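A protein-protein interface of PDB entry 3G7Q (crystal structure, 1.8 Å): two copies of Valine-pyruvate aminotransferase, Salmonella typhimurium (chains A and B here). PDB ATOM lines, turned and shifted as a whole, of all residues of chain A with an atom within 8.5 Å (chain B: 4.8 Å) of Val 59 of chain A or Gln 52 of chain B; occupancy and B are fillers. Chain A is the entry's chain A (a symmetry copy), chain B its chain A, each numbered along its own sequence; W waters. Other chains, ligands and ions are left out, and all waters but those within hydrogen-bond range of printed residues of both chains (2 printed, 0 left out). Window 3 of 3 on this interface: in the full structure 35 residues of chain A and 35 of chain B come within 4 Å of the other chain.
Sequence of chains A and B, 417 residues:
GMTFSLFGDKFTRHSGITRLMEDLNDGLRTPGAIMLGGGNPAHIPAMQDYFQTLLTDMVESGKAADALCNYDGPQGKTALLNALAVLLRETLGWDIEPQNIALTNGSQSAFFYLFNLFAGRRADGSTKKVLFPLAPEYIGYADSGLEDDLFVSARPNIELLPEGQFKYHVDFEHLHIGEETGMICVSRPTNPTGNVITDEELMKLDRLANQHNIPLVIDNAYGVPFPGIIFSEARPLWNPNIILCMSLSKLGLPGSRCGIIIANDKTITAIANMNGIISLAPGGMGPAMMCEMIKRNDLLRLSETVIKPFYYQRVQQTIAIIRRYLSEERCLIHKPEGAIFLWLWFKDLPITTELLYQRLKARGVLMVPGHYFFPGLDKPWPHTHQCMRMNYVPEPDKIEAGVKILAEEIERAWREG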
ATOM      1  N   PHE A  51      -6.600 -12.912 -29.457  1.00  0.00           N
ATOM      2  CA  PHE A  51      -6.741 -13.659 -28.192  1.00  0.00           C
ATOM      3  C   PHE A  51      -6.700 -12.760 -26.963  1.00  0.00           C
ATOM      4  O   PHE A  51      -7.413 -13.015 -25.976  1.00  0.00           O
ATOM      5  CB  PHE A  51      -5.688 -14.748 -28.070  1.00  0.00           C
ATOM      6  CG  PHE A  51      -5.808 -15.856 -29.116  1.00  0.00           C
ATOM      7  CD1 PHE A  51      -7.018 -16.500 -29.355  1.00  0.00           C
ATOM      8  CD2 PHE A  51      -4.694 -16.316 -29.777  1.00  0.00           C
ATOM      9  CE1 PHE A  51      -7.109 -17.531 -30.295  1.00  0.00           C
ATOM     10  CE2 PHE A  51      -4.796 -17.346 -30.739  1.00  0.00           C
ATOM     11  CZ  PHE A  51      -6.012 -17.937 -30.993  1.00  0.00           C
ATOM     12  N   GLN A  52      -5.863 -11.725 -26.989  1.00  0.00           N
ATOM     13  CA  GLN A  52      -5.805 -10.798 -25.863  1.00  0.00           C
ATOM     14  C   GLN A  52      -7.150 -10.099 -25.658  1.00  0.00           C
ATOM     15  O   GLN A  52      -7.636  -9.957 -24.516  1.00  0.00           O
ATOM     16  CB  GLN A  52      -4.672  -9.786 -26.041  1.00  0.00           C
ATOM     17  CG  GLN A  52      -4.585  -8.745 -24.945  1.00  0.00           C
ATOM     18  CD  GLN A  52      -4.334  -9.335 -23.555  1.00  0.00           C
ATOM     19  OE1 GLN A  52      -3.638 -10.345 -23.411  1.00  0.00           O
ATOM     20  NE2 GLN A  52      -4.829  -8.667 -22.546  1.00  0.00           N
ATOM     21  N   THR A  53      -7.775  -9.675 -26.749  1.00  0.00           N
ATOM     22  CA  THR A  53      -9.070  -9.019 -26.652  1.00  0.00           C
ATOM     23  C   THR A  53     -10.149 -10.010 -26.216  1.00  0.00           C
ATOM     24  O   THR A  53     -10.998  -9.691 -25.399  1.00  0.00           O
ATOM     25  CB  THR A  53      -9.455  -8.368 -28.003  1.00  0.00           C
ATOM     26  OG1 THR A  53      -8.434  -7.436 -28.357  1.00  0.00           O
ATOM     27  CG2 THR A  53     -10.809  -7.652 -27.917  1.00  0.00           C
ATOM     28  N   LEU A  54     -10.117 -11.211 -26.778  1.00  0.00           N
ATOM     29  CA  LEU A  54     -11.092 -12.219 -26.415  1.00  0.00           C
ATOM     30  C   LEU A  54     -10.993 -12.555 -24.919  1.00  0.00           C
ATOM     31  O   LEU A  54     -12.004 -12.636 -24.214  1.00  0.00           O
ATOM     32  CB  LEU A  54     -10.864 -13.473 -27.224  1.00  0.00           C
ATOM     33  CG  LEU A  54     -11.837 -14.618 -26.993  1.00  0.00           C
ATOM     34  CD1 LEU A  54     -13.292 -14.197 -27.357  1.00  0.00           C
ATOM     35  CD2 LEU A  54     -11.385 -15.841 -27.776  1.00  0.00           C
ATOM     36  N   LEU A  55      -9.775 -12.762 -24.450  1.00  0.00           N
ATOM     37  CA  LEU A  55      -9.572 -13.087 -23.030  1.00  0.00           C
ATOM     38  C   LEU A  55     -10.032 -11.947 -22.142  1.00  0.00           C
ATOM     39  O   LEU A  55     -10.636 -12.165 -21.087  1.00  0.00           O
ATOM     40  CB  LEU A  55      -8.104 -13.425 -22.791  1.00  0.00           C
ATOM     41  CG  LEU A  55      -7.675 -14.791 -23.352  1.00  0.00           C
ATOM     42  CD1 LEU A  55      -6.151 -14.900 -23.374  1.00  0.00           C
ATOM     43  CD2 LEU A  55      -8.310 -15.971 -22.537  1.00  0.00           C
ATOM     44  N   THR A  56      -9.753 -10.714 -22.563  1.00  0.00           N
ATOM     45  CA  THR A  56     -10.194  -9.552 -21.806  1.00  0.00           C
ATOM     46  C   THR A  56     -11.711  -9.558 -21.684  1.00  0.00           C
ATOM     47  O   THR A  56     -12.255  -9.366 -20.579  1.00  0.00           O
ATOM     48  CB  THR A  56      -9.669  -8.239 -22.429  1.00  0.00           C
ATOM     49  OG1 THR A  56      -8.231  -8.226 -22.341  1.00  0.00           O
ATOM     50  CG2 THR A  56     -10.261  -7.016 -21.720  1.00  0.00           C
ATOM     51  N   ASP A  57     -12.412  -9.811 -22.784  1.00  0.00           N
ATOM     52  CA  ASP A  57     -13.882  -9.850 -22.750  1.00  0.00           C
ATOM     53  C   ASP A  57     -14.412 -10.978 -21.873  1.00  0.00           C
ATOM     54  O   ASP A  57     -15.364 -10.796 -21.118  1.00  0.00           O
ATOM     55  CB  ASP A  57     -14.463 -10.059 -24.147  1.00  0.00           C
ATOM     56  CG  ASP A  57     -14.206  -8.888 -25.085  1.00  0.00           C
ATOM     57  OD1 ASP A  57     -13.883  -7.775 -24.629  1.00  0.00           O
ATOM     58  OD2 ASP A  57     -14.333  -9.100 -26.296  1.00  0.00           O
ATOM     59  N   MET A  58     -13.793 -12.151 -22.010  1.00  0.00           N
ATOM     60  CA  MET A  58     -14.210 -13.333 -21.250  1.00  0.00           C
ATOM     61  C   MET A  58     -13.975 -13.199 -19.757  1.00  0.00           C
ATOM     62  O   MET A  58     -14.802 -13.655 -18.975  1.00  0.00           O
ATOM     63  CB  MET A  58     -13.533 -14.594 -21.796  1.00  0.00           C
ATOM     64  CG  MET A  58     -14.003 -14.964 -23.187  1.00  0.00           C
ATOM     65  SD  MET A  58     -13.073 -16.512 -23.873  1.00  0.00           S
ATOM     66  CE  MET A  58     -13.817 -17.921 -22.610  1.00  0.00           C
ATOM     67  N   VAL A  59     -12.869 -12.585 -19.356  1.00  0.00           N
ATOM     68  CA  VAL A  59     -12.628 -12.381 -17.938  1.00  0.00           C
ATOM     69  C   VAL A  59     -13.641 -11.373 -17.394  1.00  0.00           C
ATOM     70  O   VAL A  59     -14.240 -11.595 -16.337  1.00  0.00           O
ATOM     71  CB  VAL A  59     -11.207 -11.917 -17.647  1.00  0.00           C
ATOM     72  CG1 VAL A  59     -11.071 -11.574 -16.172  1.00  0.00           C
ATOM     73  CG2 VAL A  59     -10.214 -13.004 -18.032  1.00  0.00           C
ATOM     74  N   GLU A  60     -13.868 -10.293 -18.142  1.00  0.00           N
ATOM     75  CA  GLU A  60     -14.819  -9.248 -17.713  1.00  0.00           C
ATOM     76  C   GLU A  60     -16.265  -9.748 -17.640  1.00  0.00           C
ATOM     77  O   GLU A  60     -17.017  -9.318 -16.776  1.00  0.00           O
ATOM     78  CB  GLU A  60     -14.708  -8.004 -18.618  1.00  0.00           C
ATOM     79  CG  GLU A  60     -13.370  -7.263 -18.438  1.00  0.00           C
ATOM     80  CD  GLU A  60     -13.129  -6.062 -19.393  1.00  0.00           C
ATOM     81  OE1 GLU A  60     -13.898  -5.859 -20.367  1.00  0.00           O
ATOM     82  OE2 GLU A  60     -12.134  -5.333 -19.151  1.00  0.00           O
ATOM     83  N   SER A  61     -16.645 -10.688 -18.501  1.00  0.00           N
ATOM     84  CA  SER A  61     -18.023 -11.205 -18.488  1.00  0.00           C
ATOM     85  C   SER A  61     -18.250 -12.339 -17.494  1.00  0.00           C
ATOM     86  O   SER A  61     -19.393 -12.782 -17.329  1.00  0.00           O
ATOM     87  CB  SER A  61     -18.404 -11.705 -19.874  1.00  0.00           C
ATOM     88  OG  SER A  61     -17.646 -12.845 -20.233  1.00  0.00           O
ATOM     89  N   GLY A  62     -17.189 -12.812 -16.829  1.00  0.00           N
ATOM     90  CA  GLY A  62     -17.316 -13.936 -15.884  1.00  0.00           C
ATOM     91  C   GLY A  62     -17.083 -15.289 -16.555  1.00  0.00           C
ATOM     92  O   GLY A  62     -17.020 -16.321 -15.876  1.00  0.00           O
ATOM     93  N   LYS A  63     -16.937 -15.305 -17.873  1.00  0.00           N
ATOM     94  CA  LYS A  63     -16.786 -16.569 -18.608  1.00  0.00           C
ATOM     95  C   LYS A  63     -15.470 -17.300 -18.345  1.00  0.00           C
ATOM     96  O   LYS A  63     -15.458 -18.537 -18.327  1.00  0.00           O
ATOM     97  CB  LYS A  63     -16.978 -16.357 -20.092  1.00  0.00           C
ATOM     98  CG  LYS A  63     -18.408 -15.963 -20.483  1.00  0.00           C
ATOM     99  CD  LYS A  63     -18.443 -15.599 -21.960  1.00  0.00           C
ATOM    100  CE  LYS A  63     -19.806 -15.075 -22.410  1.00  0.00           C
ATOM    101  NZ  LYS A  63     -19.741 -14.492 -23.795  1.00  0.00           N
ATOM    102  N   ALA A  64     -14.381 -16.560 -18.109  1.00  0.00           N
ATOM    103  CA  ALA A  64     -13.101 -17.188 -17.830  1.00  0.00           C
ATOM    104  C   ALA A  64     -13.175 -17.892 -16.481  1.00  0.00           C
ATOM    105  O   ALA A  64     -12.766 -19.051 -16.346  1.00  0.00           O
ATOM    106  CB  ALA A  64     -11.968 -16.170 -17.838  1.00  0.00           C
ATOM    107  N   ALA A  65     -13.712 -17.191 -15.487  1.00  0.00           N
ATOM    108  CA  ALA A  65     -13.874 -17.770 -14.163  1.00  0.00           C
ATOM    109  C   ALA A  65     -14.799 -18.983 -14.227  1.00  0.00           C
ATOM    110  O   ALA A  65     -14.523 -19.994 -13.584  1.00  0.00           O
ATOM    111  CB  ALA A  65     -14.397 -16.732 -13.157  1.00  0.00           C
ATOM    112  N   ASP A  66     -15.880 -18.901 -15.003  1.00  0.00           N
ATOM    113  CA  ASP A  66     -16.809 -20.036 -15.128  1.00  0.00           C
ATOM    114  C   ASP A  66     -16.088 -21.276 -15.687  1.00  0.00           C
ATOM    115  O   ASP A  66     -16.320 -22.399 -15.245  1.00  0.00           O
ATOM    116  CB  ASP A  66     -17.969 -19.714 -16.059  1.00  0.00           C
ATOM    117  CG  ASP A  66     -18.996 -18.776 -15.465  1.00  0.00           C
ATOM    118  OD1 ASP A  66     -18.996 -18.524 -14.242  1.00  0.00           O
ATOM    119  OD2 ASP A  66     -19.844 -18.297 -16.260  1.00  0.00           O
ATOM    120  N   LEU A  68     -12.885 -22.069 -15.446  1.00  0.00           N
ATOM    121  CA  LEU A  68     -11.904 -22.643 -14.534  1.00  0.00           C
ATOM    122  C   LEU A  68     -12.501 -23.150 -13.241  1.00  0.00           C
ATOM    123  O   LEU A  68     -12.009 -24.129 -12.667  1.00  0.00           O
ATOM    124  CB  LEU A  68     -10.814 -21.597 -14.246  1.00  0.00           C
ATOM    125  CG  LEU A  68      -9.964 -21.196 -15.453  1.00  0.00           C
ATOM    126  CD1 LEU A  68      -9.281 -19.852 -15.249  1.00  0.00           C
ATOM    127  CD2 LEU A  68      -8.947 -22.278 -15.771  1.00  0.00           C
ATOM    128  N   CYS A  69     -13.558 -22.491 -12.763  1.00  0.00           N
ATOM    129  CA  CYS A  69     -14.154 -22.818 -11.484  1.00  0.00           C
ATOM    130  C   CYS A  69     -15.273 -23.855 -11.505  1.00  0.00           C
ATOM    131  O   CYS A  69     -15.769 -24.215 -10.444  1.00  0.00           O
ATOM    132  CB  CYS A  69     -14.645 -21.542 -10.801  1.00  0.00           C
ATOM    133  SG  CYS A  69     -13.247 -20.382 -10.518  1.00  0.00           S
ATOM    134  N   MET A 285     -10.584 -23.827 -20.248  1.00  0.00           N
ATOM    135  CA  MET A 285     -10.334 -22.593 -20.973  1.00  0.00           C
ATOM    136  C   MET A 285     -10.413 -22.771 -22.515  1.00  0.00           C
ATOM    137  O   MET A 285     -11.034 -21.960 -23.203  1.00  0.00           O
ATOM    138  CB  MET A 285      -9.004 -22.016 -20.526  1.00  0.00           C
ATOM    139  CG  MET A 285      -8.931 -20.541 -20.651  1.00  0.00           C
ATOM    140  SD  MET A 285     -10.210 -19.604 -19.480  1.00  0.00           S
ATOM    141  CE  MET A 285     -10.304 -18.354 -20.649  1.00  0.00           C
ATOM    142  N   ARG A 296     -19.101 -16.092 -32.104  1.00  0.00           N
ATOM    143  CA  ARG A 296     -18.778 -14.835 -32.758  1.00  0.00           C
ATOM    144  C   ARG A 296     -18.490 -14.981 -34.257  1.00  0.00           C
ATOM    145  O   ARG A 296     -18.195 -13.984 -34.917  1.00  0.00           O
ATOM    146  CB  ARG A 296     -17.572 -14.199 -32.084  1.00  0.00           C
ATOM    147  CG  ARG A 296     -17.783 -13.870 -30.626  1.00  0.00           C
ATOM    148  CD  ARG A 296     -16.539 -13.299 -30.020  1.00  0.00           C
ATOM    149  NE  ARG A 296     -16.788 -13.000 -28.607  1.00  0.00           N
ATOM    150  CZ  ARG A 296     -16.113 -12.104 -27.889  1.00  0.00           C
ATOM    151  NH1 ARG A 296     -15.156 -11.349 -28.432  1.00  0.00           N
ATOM    152  NH2 ARG A 296     -16.429 -11.930 -26.616  1.00  0.00           N
ATOM    153  N   GLN B  48     -14.257 -17.407  -5.176  1.00  0.00           N
ATOM    154  CA  GLN B  48     -14.682 -16.969  -6.514  1.00  0.00           C
ATOM    155  C   GLN B  48     -14.269 -15.520  -6.738  1.00  0.00           C
ATOM    156  O   GLN B  48     -13.770 -15.165  -7.816  1.00  0.00           O
ATOM    157  CB  GLN B  48     -16.177 -17.156  -6.685  1.00  0.00           C
ATOM    158  CG  GLN B  48     -16.654 -18.623  -6.597  1.00  0.00           C
ATOM    159  CD  GLN B  48     -16.166 -19.537  -7.725  1.00  0.00           C
ATOM    160  OE1 GLN B  48     -16.269 -20.761  -7.627  1.00  0.00           O
ATOM    161  NE2 GLN B  48     -15.662 -18.947  -8.809  1.00  0.00           N
ATOM    162  N   ASP B  49     -14.416 -14.686  -5.707  1.00  0.00           N
ATOM    163  CA  ASP B  49     -13.990 -13.291  -5.801  1.00  0.00           C
ATOM    164  C   ASP B  49     -12.476 -13.204  -6.006  1.00  0.00           C
ATOM    165  O   ASP B  49     -11.999 -12.435  -6.842  1.00  0.00           O
ATOM    166  CB  ASP B  49     -14.362 -12.509  -4.522  1.00  0.00           C
ATOM    167  CG  ASP B  49     -15.864 -12.329  -4.340  1.00  0.00           C
ATOM    168  OD1 ASP B  49     -16.652 -12.540  -5.294  1.00  0.00           O
ATOM    169  OD2 ASP B  49     -16.256 -11.951  -3.211  1.00  0.00           O
ATOM    170  N   TYR B  50     -11.728 -13.991  -5.237  1.00  0.00           N
ATOM    171  CA  TYR B  50     -10.279 -14.035  -5.368  1.00  0.00           C
ATOM    172  C   TYR B  50      -9.869 -14.426  -6.787  1.00  0.00           C
ATOM    173  O   TYR B  50      -9.066 -13.748  -7.400  1.00  0.00           O
ATOM    174  CB  TYR B  50      -9.656 -15.035  -4.382  1.00  0.00           C
ATOM    175  CG  TYR B  50      -8.169 -15.120  -4.567  1.00  0.00           C
ATOM    176  CD1 TYR B  50      -7.310 -14.216  -3.931  1.00  0.00           C
ATOM    177  CD2 TYR B  50      -7.612 -16.084  -5.407  1.00  0.00           C
ATOM    178  CE1 TYR B  50      -5.942 -14.282  -4.126  1.00  0.00           C
ATOM    179  CE2 TYR B  50      -6.257 -16.139  -5.620  1.00  0.00           C
ATOM    180  CZ  TYR B  50      -5.422 -15.254  -4.977  1.00  0.00           C
ATOM    181  OH  TYR B  50      -4.071 -15.340  -5.197  1.00  0.00           O
ATOM    182  N   PHE B  51     -10.418 -15.522  -7.307  1.00  0.00           N
ATOM    183  CA  PHE B  51     -10.058 -15.951  -8.673  1.00  0.00           C
ATOM    184  C   PHE B  51     -10.454 -14.936  -9.738  1.00  0.00           C
ATOM    185  O   PHE B  51      -9.728 -14.753 -10.731  1.00  0.00           O
ATOM    186  CB  PHE B  51     -10.658 -17.307  -9.005  1.00  0.00           C
ATOM    187  CG  PHE B  51     -10.119 -18.456  -8.152  1.00  0.00           C
ATOM    188  CD1 PHE B  51      -8.752 -18.657  -7.987  1.00  0.00           C
ATOM    189  CD2 PHE B  51     -10.975 -19.385  -7.611  1.00  0.00           C
ATOM    190  CE1 PHE B  51      -8.271 -19.728  -7.226  1.00  0.00           C
ATOM    191  CE2 PHE B  51     -10.483 -20.455  -6.829  1.00  0.00           C
ATOM    192  CZ  PHE B  51      -9.130 -20.607  -6.639  1.00  0.00           C
ATOM    193  N   GLN B  52     -11.604 -14.285  -9.567  1.00  0.00           N
ATOM    194  CA  GLN B  52     -12.023 -13.269 -10.526  1.00  0.00           C
ATOM    195  C   GLN B  52     -11.021 -12.114 -10.572  1.00  0.00           C
ATOM    196  O   GLN B  52     -10.653 -11.621 -11.660  1.00  0.00           O
ATOM    197  CB  GLN B  52     -13.436 -12.770 -10.218  1.00  0.00           C
ATOM    198  CG  GLN B  52     -13.921 -11.664 -11.130  1.00  0.00           C
ATOM    199  CD  GLN B  52     -13.988 -12.067 -12.606  1.00  0.00           C
ATOM    200  OE1 GLN B  52     -14.282 -13.219 -12.935  1.00  0.00           O
ATOM    201  NE2 GLN B  52     -13.794 -11.109 -13.474  1.00  0.00           N
ATOM    202  N   THR B  53     -10.555 -11.679  -9.407  1.00  0.00           N
ATOM    203  CA  THR B  53      -9.583 -10.599  -9.355  1.00  0.00           C
ATOM    204  C   THR B  53      -8.236 -11.054  -9.916  1.00  0.00           C
ATOM    205  O   THR B  53      -7.581 -10.324 -10.642  1.00  0.00           O
ATOM    206  CB  THR B  53      -9.413 -10.086  -7.904  1.00  0.00           C
ATOM    207  OG1 THR B  53     -10.688  -9.651  -7.433  1.00  0.00           O
ATOM    208  CG2 THR B  53      -8.406  -8.931  -7.829  1.00  0.00           C
ATOM    209  N   LEU B  54      -7.820 -12.263  -9.560  1.00  0.00           N
ATOM    210  CA  LEU B  54      -6.562 -12.783 -10.055  1.00  0.00           C
ATOM    211  C   LEU B  54      -6.580 -12.881 -11.588  1.00  0.00           C
ATOM    212  O   LEU B  54      -5.629 -12.480 -12.265  1.00  0.00           O
ATOM    213  CB  LEU B  54      -6.303 -14.152  -9.470  1.00  0.00           C
ATOM    214  CG  LEU B  54      -4.994 -14.820  -9.858  1.00  0.00           C
ATOM    215  CD1 LEU B  54      -3.774 -13.974  -9.385  1.00  0.00           C
ATOM    216  CD2 LEU B  54      -4.956 -16.235  -9.301  1.00  0.00           C
ATOM    217  N   LEU B  55      -7.659 -13.428 -12.121  1.00  0.00           N
ATOM    218  CA  LEU B  55      -7.776 -13.565 -13.581  1.00  0.00           C
ATOM    219  C   LEU B  55      -7.780 -12.207 -14.254  1.00  0.00           C
ATOM    220  O   LEU B  55      -7.170 -12.019 -15.313  1.00  0.00           O
ATOM    221  CB  LEU B  55      -9.033 -14.360 -13.917  1.00  0.00           C
ATOM    222  CG  LEU B  55      -8.931 -15.861 -13.603  1.00  0.00           C
ATOM    223  CD1 LEU B  55     -10.315 -16.507 -13.645  1.00  0.00           C
ATOM    224  CD2 LEU B  55      -7.942 -16.586 -14.581  1.00  0.00           C
ATOM    225  N   THR B  56      -8.467 -11.241 -13.644  1.00  0.00           N
ATOM    226  CA  THR B  56      -8.491  -9.891 -14.186  1.00  0.00           C
ATOM    227  C   THR B  56      -7.076  -9.336 -14.261  1.00  0.00           C
ATOM    228  O   THR B  56      -6.670  -8.783 -15.301  1.00  0.00           O
ATOM    229  CB  THR B  56      -9.430  -8.973 -13.372  1.00  0.00           C
ATOM    230  OG1 THR B  56     -10.781  -9.458 -13.500  1.00  0.00           O
ATOM    231  CG2 THR B  56      -9.334  -7.519 -13.851  1.00  0.00           C
ATOM    232  N   VAL B  59      -4.988 -11.324 -17.020  1.00  0.00           N
ATOM    233  CA  VAL B  59      -5.329 -10.988 -18.391  1.00  0.00           C
ATOM    234  C   VAL B  59      -4.758  -9.611 -18.730  1.00  0.00           C
ATOM    235  O   VAL B  59      -4.153  -9.427 -19.791  1.00  0.00           O
ATOM    236  CB  VAL B  59      -6.830 -11.020 -18.645  1.00  0.00           C
ATOM    237  CG1 VAL B  59      -7.125 -10.509 -20.047  1.00  0.00           C
ATOM    238  CG2 VAL B  59      -7.358 -12.437 -18.476  1.00  0.00           C
HETATM  239  O   HOH W   1     -14.049 -14.208 -15.388  1.00  0.00           O
HETATM  240  O   HOH W   2      -3.429 -11.742 -21.162  1.00  0.00           O
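Of the printed residues of chain B, Val 59 of chain A touches Gln 52 (2.9 Å), Leu 55 (3.9 Å), Thr 56 (3.4 Å) and Val 59 (2.9 Å). Printed residues of chain B within 4 Å of Leu 68 of chain A: Leu 55. Of the printed residues of chain B, Cys 69 of chain A touches Gln 48 (3.3 Å) and Phe 51 (3.8 Å). Printed residues of chain A within 4 Å of Gln 48 of chain B: Cys 69. Printed residues of chain A within 4 Å of Gln 52 of chain B: Val 59 and Ala 65. Leu 54 of chain B touches none of the printed residues of chain A. The nearest printed residue of chain B that does not touch Val 59 of chain A is Phe 51 of chain B (6.4 Å).
Hydrophobic or aromatic side chains of chain A that line the printed part of chain B: Val 59, Ala 65 and Leu 68. Of the 10 printed residues of chain B, 6 touch a printed residue of chain A. Printed residues of chain B that touch a printed residue of chain A: Gln 48, Phe 51, Gln 52, Leu 55, Thr 56 and Val 59. Hydrophobic or aromatic side chains of chain B within 4 Å of the printed part of chain A: Phe 51, Leu 55 and Val 59. Among the printed residues, 12 pairs touch across the chains. Among the printed residues, no Asp or Glu carboxylate lies within 4 Å of a Lys or Arg side-chain nitrogen of the other chain.
The backbone carbonyl oxygen (O) of Gln 52 of chain B sits at hydrogen-bond distance from the side-chain hydroxyl (OG1) of Thr 56 of chain B (2.8 Å). O of Gln 52 of chain A sits at hydrogen-bond distance from OG1 of Thr 56 of chain A (2.8 Å). SG of Cys 69 of chain A sits close to O of Ala 65 of chain A (3.3 Å).
Gln 52 of chain A touches Val 59 of chain B, and with the chains exchanged Val 59 of chain A touches Gln 52 of chain B. Leu 55 of chain A touches Val 59 of chain B, and with the chains exchanged Val 59 of chain A touches Leu 55 of chain B. Thr 56 of chain A touches Val 59 of chain B, and with the chains exchanged Val 59 of chain A touches Thr 56 of chain B. Val 59 of chain B touches its own counterpart, Val 59 of chain A. Positions printed for both chains: 51, 52, 53, 54, 55, 56 and 59. Of the 12 pairs that touch across the chains among the printed residues, 7 have their exchanged pair printed and touching as well.
Val 59 of chain B touches Leu 55 of chain A. Thr 56 of chain A touches Val 59 of chain B (OG1 to CG1, 3.4 Å). Val 59 of chain A touches Leu 55 of chain B. OG1 of Thr 56 of chain B touches CG1 of Val 59 of chain A (3.4 Å). CG2 of Val 59 of chain B touches CG2 of Val 59 of chain A, at 2.9 Å. OE1 of Gln 52 of chain B touches CB of Ala 65 of chain A (3.5 Å). Ala 65 of chain A touches Leu 55 of chain B (CA to CD1, 3.8 Å). CD1 of Leu 68 of chain A touches CD2 of Leu 55 of chain B, 3.6 Å away. Cys 69 of chain A touches Phe 51 of chain B (SG to CD2, 3.8 Å).
Water W2 bridges the side-chain amide oxygen of Gln 52 of chain A (2.7 Å) and the backbone carbonyl oxygen of Val 59 of chain B (2.8 Å). Water W1 lies within hydrogen-bond range of OE1 of Gln 52 of chain B (2.7 Å), O of Val 59 of chain A (2.8 Å) and N of Ala 65 of chain A (3.0 Å).
The side-chain amide nitrogen (NE2) of Gln 48 of chain B sits at hydrogen-bond distance from the side-chain sulfur (SG) of Cys 69 of chain A (3.3 Å). The side-chain amide nitrogen (NE2) of Gln 52 of chain B is in hydrogen-bond range of the backbone carbonyl oxygen (O) of Val 59 of chain A, at 2.9 Å. The side-chain amide nitrogen (NE2) of Gln 52 of chain A lies within hydrogen-bond range of the backbone carbonyl oxygen (O) of Val 59 of chain B.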
